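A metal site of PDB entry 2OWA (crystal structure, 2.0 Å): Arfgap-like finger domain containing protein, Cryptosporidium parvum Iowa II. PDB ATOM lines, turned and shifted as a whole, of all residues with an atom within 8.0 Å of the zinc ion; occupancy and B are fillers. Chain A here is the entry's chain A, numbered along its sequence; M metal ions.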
ATOM      1  N   THR A  38      14.159 -14.649 -17.911  1.00  0.00           N
ATOM      2  CA  THR A  38      14.043 -13.328 -18.464  1.00  0.00           C
ATOM      3  C   THR A  38      14.481 -12.310 -17.379  1.00  0.00           C
ATOM      4  O   THR A  38      14.232 -12.528 -16.202  1.00  0.00           O
ATOM      5  CB  THR A  38      12.599 -13.136 -18.924  1.00  0.00           C
ATOM      6  OG1 THR A  38      12.422 -11.818 -19.420  1.00  0.00           O
ATOM      7  CG2 THR A  38      11.634 -13.356 -17.788  1.00  0.00           C
ATOM      8  N   CYS A  39      15.163 -11.236 -17.752  1.00  0.00           N
ATOM      9  CA  CYS A  39      15.656 -10.248 -16.763  1.00  0.00           C
ATOM     10  C   CYS A  39      14.490  -9.665 -15.965  1.00  0.00           C
ATOM     11  O   CYS A  39      13.449  -9.347 -16.534  1.00  0.00           O
ATOM     12  CB  CYS A  39      16.405  -9.133 -17.479  1.00  0.00           C
ATOM     13  SG  CYS A  39      16.737  -7.653 -16.544  1.00  0.00           S
ATOM     14  N   PHE A  40      14.681  -9.498 -14.663  1.00  0.00           N
ATOM     15  CA  PHE A  40      13.627  -8.955 -13.800  1.00  0.00           C
ATOM     16  C   PHE A  40      13.197  -7.538 -14.222  1.00  0.00           C
ATOM     17  O   PHE A  40      12.022  -7.179 -14.085  1.00  0.00           O
ATOM     18  CB  PHE A  40      14.069  -8.954 -12.320  1.00  0.00           C
ATOM     19  CG  PHE A  40      12.939  -8.625 -11.356  1.00  0.00           C
ATOM     20  CD1 PHE A  40      11.955  -9.567 -11.075  1.00  0.00           C
ATOM     21  CD2 PHE A  40      12.889  -7.389 -10.727  1.00  0.00           C
ATOM     22  CE1 PHE A  40      10.891  -9.267 -10.193  1.00  0.00           C
ATOM     23  CE2 PHE A  40      11.820  -7.092  -9.825  1.00  0.00           C
ATOM     24  CZ  PHE A  40      10.835  -8.058  -9.580  1.00  0.00           C
ATOM     25  N   ASP A  41      14.145  -6.735 -14.715  1.00  0.00           N
ATOM     26  CA  ASP A  41      13.831  -5.341 -15.089  1.00  0.00           C
ATOM     27  C   ASP A  41      13.326  -5.148 -16.520  1.00  0.00           C
ATOM     28  O   ASP A  41      12.367  -4.390 -16.739  1.00  0.00           O
ATOM     29  CB  ASP A  41      15.046  -4.435 -14.881  1.00  0.00           C
ATOM     30  CG  ASP A  41      15.464  -4.305 -13.428  1.00  0.00           C
ATOM     31  OD1 ASP A  41      14.900  -5.050 -12.577  1.00  0.00           O
ATOM     32  OD2 ASP A  41      16.363  -3.469 -13.152  1.00  0.00           O
ATOM     33  N   CYS A  42      13.952  -5.809 -17.491  1.00  0.00           N
ATOM     34  CA  CYS A  42      13.655  -5.520 -18.891  1.00  0.00           C
ATOM     35  C   CYS A  42      13.247  -6.705 -19.754  1.00  0.00           C
ATOM     36  O   CYS A  42      13.021  -6.551 -20.957  1.00  0.00           O
ATOM     37  CB  CYS A  42      14.832  -4.811 -19.537  1.00  0.00           C
ATOM     38  SG  CYS A  42      16.120  -5.947 -20.071  1.00  0.00           S
ATOM     39  N   GLU A  43      13.217  -7.896 -19.168  1.00  0.00           N
ATOM     40  CA  GLU A  43      12.836  -9.116 -19.882  1.00  0.00           C
ATOM     41  C   GLU A  43      13.795  -9.635 -21.010  1.00  0.00           C
ATOM     42  O   GLU A  43      13.438 -10.590 -21.725  1.00  0.00           O
ATOM     43  CB  GLU A  43      11.350  -9.057 -20.315  1.00  0.00           C
ATOM     44  CG  GLU A  43      10.379  -8.651 -19.168  1.00  0.00           C
ATOM     45  CD  GLU A  43       8.906  -8.760 -19.520  1.00  0.00           C
ATOM     46  OE1 GLU A  43       8.447  -8.177 -20.535  1.00  0.00           O
ATOM     47  OE2 GLU A  43       8.161  -9.425 -18.746  1.00  0.00           O
ATOM     48  N   SER A  44      14.969  -9.017 -21.158  1.00  0.00           N
ATOM     49  CA  SER A  44      16.091  -9.568 -21.921  1.00  0.00           C
ATOM     50  C   SER A  44      16.290 -10.999 -21.470  1.00  0.00           C
ATOM     51  O   SER A  44      16.178 -11.302 -20.291  1.00  0.00           O
ATOM     52  CB  SER A  44      17.374  -8.733 -21.685  1.00  0.00           C
ATOM     53  OG  SER A  44      18.562  -9.411 -22.094  1.00  0.00           O
ATOM     54  N   ARG A  45      16.595 -11.892 -22.412  1.00  0.00           N
ATOM     55  CA  ARG A  45      16.518 -13.326 -22.154  1.00  0.00           C
ATOM     56  C   ARG A  45      17.794 -13.891 -21.540  1.00  0.00           C
ATOM     57  O   ARG A  45      18.857 -13.349 -21.753  1.00  0.00           O
ATOM     58  CB  ARG A  45      16.060 -14.040 -23.434  1.00  0.00           C
ATOM     59  CG  ARG A  45      14.655 -13.553 -23.833  1.00  0.00           C
ATOM     60  CD  ARG A  45      14.551 -13.071 -25.293  1.00  0.00           C
ATOM     61  NE  ARG A  45      14.195 -14.188 -26.162  1.00  0.00           N
ATOM     62  CZ  ARG A  45      13.078 -14.314 -26.871  1.00  0.00           C
ATOM     63  NH1 ARG A  45      12.161 -13.347 -26.906  1.00  0.00           N
ATOM     64  NH2 ARG A  45      12.894 -15.422 -27.575  1.00  0.00           N
ATOM     65  N   PRO A  47      19.108 -13.968 -18.288  1.00  0.00           N
ATOM     66  CA  PRO A  47      19.959 -13.050 -17.516  1.00  0.00           C
ATOM     67  C   PRO A  47      20.915 -13.845 -16.600  1.00  0.00           C
ATOM     68  O   PRO A  47      20.547 -14.908 -16.063  1.00  0.00           O
ATOM     69  CB  PRO A  47      18.952 -12.250 -16.679  1.00  0.00           C
ATOM     70  CG  PRO A  47      17.851 -13.266 -16.422  1.00  0.00           C
ATOM     71  CD  PRO A  47      17.724 -13.974 -17.767  1.00  0.00           C
ATOM     72  N   PHE A  57      17.317 -12.176 -10.808  1.00  0.00           N
ATOM     73  CA  PHE A  57      18.272 -12.219 -11.940  1.00  0.00           C
ATOM     74  C   PHE A  57      17.995 -11.134 -12.966  1.00  0.00           C
ATOM     75  O   PHE A  57      16.836 -10.918 -13.344  1.00  0.00           O
ATOM     76  CB  PHE A  57      18.239 -13.561 -12.642  1.00  0.00           C
ATOM     77  CG  PHE A  57      18.710 -14.676 -11.799  1.00  0.00           C
ATOM     78  CD1 PHE A  57      20.048 -15.026 -11.784  1.00  0.00           C
ATOM     79  CD2 PHE A  57      17.804 -15.380 -10.993  1.00  0.00           C
ATOM     80  CE1 PHE A  57      20.501 -16.085 -10.957  1.00  0.00           C
ATOM     81  CE2 PHE A  57      18.223 -16.421 -10.183  1.00  0.00           C
ATOM     82  CZ  PHE A  57      19.568 -16.797 -10.181  1.00  0.00           C
ATOM     83  N   ILE A  58      19.065 -10.480 -13.431  1.00  0.00           N
ATOM     84  CA  ILE A  58      18.981  -9.295 -14.302  1.00  0.00           C
ATOM     85  C   ILE A  58      20.069  -9.385 -15.384  1.00  0.00           C
ATOM     86  O   ILE A  58      21.038 -10.084 -15.173  1.00  0.00           O
ATOM     87  CB  ILE A  58      19.153  -7.979 -13.481  1.00  0.00           C
ATOM     88  CG1 ILE A  58      20.464  -7.989 -12.637  1.00  0.00           C
ATOM     89  CG2 ILE A  58      17.856  -7.693 -12.634  1.00  0.00           C
ATOM     90  CD1 ILE A  58      20.698  -6.686 -11.865  1.00  0.00           C
ATOM     91  N   CYS A  59      19.927  -8.671 -16.499  1.00  0.00           N
ATOM     92  CA  CYS A  59      20.879  -8.777 -17.590  1.00  0.00           C
ATOM     93  C   CYS A  59      22.094  -7.866 -17.360  1.00  0.00           C
ATOM     94  O   CYS A  59      22.118  -7.044 -16.445  1.00  0.00           O
ATOM     95  CB  CYS A  59      20.203  -8.463 -18.953  1.00  0.00           C
ATOM     96  SG  CYS A  59      19.584  -6.738 -19.154  1.00  0.00           S
ATOM     97  N   LEU A  60      23.078  -8.022 -18.240  1.00  0.00           N
ATOM     98  CA  LEU A  60      24.321  -7.258 -18.186  1.00  0.00           C
ATOM     99  C   LEU A  60      24.070  -5.763 -18.293  1.00  0.00           C
ATOM    100  O   LEU A  60      24.781  -4.958 -17.674  1.00  0.00           O
ATOM    101  CB  LEU A  60      25.320  -7.793 -19.243  1.00  0.00           C
ATOM    102  CG  LEU A  60      24.961  -7.922 -20.742  1.00  0.00           C
ATOM    103  CD1 LEU A  60      24.863  -6.543 -21.384  1.00  0.00           C
ATOM    104  CD2 LEU A  60      25.971  -8.776 -21.545  1.00  0.00           C
ATOM    105  N   ASN A  61      23.032  -5.377 -19.050  1.00  0.00           N
ATOM    106  CA  ASN A  61      22.602  -3.989 -19.183  1.00  0.00           C
ATOM    107  C   ASN A  61      22.021  -3.481 -17.847  1.00  0.00           C
ATOM    108  O   ASN A  61      22.511  -2.498 -17.290  1.00  0.00           O
ATOM    109  CB  ASN A  61      21.566  -3.874 -20.322  1.00  0.00           C
ATOM    110  CG  ASN A  61      21.408  -2.449 -20.836  1.00  0.00           C
ATOM    111  OD1 ASN A  61      20.817  -1.570 -20.176  1.00  0.00           O
ATOM    112  ND2 ASN A  61      21.922  -2.209 -22.062  1.00  0.00           N
ATOM    113  N   CYS A  62      21.033  -4.180 -17.315  1.00  0.00           N
ATOM    114  CA  CYS A  62      20.384  -3.731 -16.071  1.00  0.00           C
ATOM    115  C   CYS A  62      21.325  -3.811 -14.878  1.00  0.00           C
ATOM    116  O   CYS A  62      21.221  -2.994 -13.978  1.00  0.00           O
ATOM    117  CB  CYS A  62      19.066  -4.482 -15.807  1.00  0.00           C
ATOM    118  SG  CYS A  62      17.900  -4.126 -17.141  1.00  0.00           S
ATOM    119  N   SER A  63      22.273  -4.765 -14.906  1.00  0.00           N
ATOM    120  CA  SER A  63      23.303  -4.875 -13.872  1.00  0.00           C
ATOM    121  C   SER A  63      24.148  -3.616 -13.706  1.00  0.00           C
ATOM    122  O   SER A  63      24.451  -3.234 -12.579  1.00  0.00           O
ATOM    123  CB  SER A  63      24.201  -6.086 -14.116  1.00  0.00           C
ATOM    124  OG  SER A  63      24.922  -5.940 -15.343  1.00  0.00           O
ATOM    125  N   ASP A  65      23.191  -0.428 -14.454  1.00  0.00           N
ATOM    126  CA  ASP A  65      22.304   0.508 -13.729  1.00  0.00           C
ATOM    127  C   ASP A  65      22.241   0.247 -12.234  1.00  0.00           C
ATOM    128  O   ASP A  65      22.368   1.182 -11.439  1.00  0.00           O
ATOM    129  CB  ASP A  65      20.891   0.533 -14.315  1.00  0.00           C
ATOM    130  CG  ASP A  65      20.874   0.940 -15.806  1.00  0.00           C
ATOM    131  OD1 ASP A  65      21.778   1.673 -16.271  1.00  0.00           O
ATOM    132  OD2 ASP A  65      19.968   0.460 -16.518  1.00  0.00           O
ATOM    133  N   HIS A  66      22.024  -1.016 -11.859  1.00  0.00           N
ATOM    134  CA  HIS A  66      22.025  -1.408 -10.444  1.00  0.00           C
ATOM    135  C   HIS A  66      23.352  -1.108  -9.741  1.00  0.00           C
ATOM    136  O   HIS A  66      23.350  -0.739  -8.585  1.00  0.00           O
ATOM    137  CB  HIS A  66      21.720  -2.891 -10.278  1.00  0.00           C
ATOM    138  CG  HIS A  66      20.269  -3.215 -10.430  1.00  0.00           C
ATOM    139  ND1 HIS A  66      19.511  -3.698  -9.397  1.00  0.00           N
ATOM    140  CD2 HIS A  66      19.447  -3.122 -11.504  1.00  0.00           C
ATOM    141  CE1 HIS A  66      18.274  -3.909  -9.818  1.00  0.00           C
ATOM    142  NE2 HIS A  66      18.206  -3.560 -11.091  1.00  0.00           N
ATOM    143  N   PRO A 114       9.377  -2.499 -13.350  1.00  0.00           N
ATOM    144  CA  PRO A 114      10.712  -2.809 -12.845  1.00  0.00           C
ATOM    145  C   PRO A 114      11.832  -2.195 -13.681  1.00  0.00           C
ATOM    146  O   PRO A 114      12.937  -2.064 -13.206  1.00  0.00           O
ATOM    147  CB  PRO A 114      10.776  -4.362 -12.884  1.00  0.00           C
ATOM    148  CG  PRO A 114       9.717  -4.766 -13.887  1.00  0.00           C
ATOM    149  CD  PRO A 114       8.643  -3.724 -13.753  1.00  0.00           C
ATOM    150  N   LYS A 115      11.526  -1.769 -14.913  1.00  0.00           N
ATOM    151  CA  LYS A 115      12.514  -1.112 -15.747  1.00  0.00           C
ATOM    152  C   LYS A 115      13.105   0.128 -15.075  1.00  0.00           C
ATOM    153  O   LYS A 115      14.244   0.436 -15.286  1.00  0.00           O
ATOM    154  CB  LYS A 115      11.923  -0.705 -17.112  1.00  0.00           C
ATOM    155  CG  LYS A 115      12.997  -0.467 -18.121  1.00  0.00           C
ATOM    156  N   LYS A 117      13.519   0.634 -11.888  1.00  0.00           N
ATOM    157  CA  LYS A 117      14.124   0.211 -10.615  1.00  0.00           C
ATOM    158  C   LYS A 117      13.573   1.015  -9.409  1.00  0.00           C
ATOM    159  O   LYS A 117      14.176   1.034  -8.324  1.00  0.00           O
ATOM    160  CB  LYS A 117      15.663   0.294 -10.669  1.00  0.00           C
ATOM    161  CG  LYS A 117      16.311  -0.501 -11.805  1.00  0.00           C
ATOM    162  CD  LYS A 117      16.766   0.383 -12.999  1.00  0.00           C
ATOM    163  CE  LYS A 117      17.438  -0.441 -14.101  1.00  0.00           C
ATOM    164  NZ  LYS A 117      16.492  -1.446 -14.767  1.00  0.00           N
HETATM  165 ZN    ZN M   1      17.571  -6.071 -18.176  1.00  0.00          ZN
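The zinc ion is bound by SG of Cys 62 (2.2 Å), SG of Cys 59 (2.3 Å), SG of Cys 42 (2.4 Å) and SG of Cys 39 (2.4 Å).
The zinc ion has four donor atoms within binding distance.
Four residues have an atom within 4 Å of the zinc ion: Cys 39, Cys 42, Cys 59 and Cys 62.
N of Asn 61 sits close to SG of Cys 59 (3.7 Å).
O of Cys 59 is in hydrogen-bond range of OG of Ser 63 (3.2 Å).
The side-chain sulfur (SG) of Cys 42 sits close to the backbone NH (N) of Ser 44 (3.5 Å).
The backbone carbonyl oxygen (O) of Ser 44 lies within hydrogen-bond range of the backbone NH (N) of Cys 39 (2.7 Å).
The side-chain sulfur (SG) of Cys 39 sits close to the backbone NH (N) of Asp 41 (3.3 Å).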
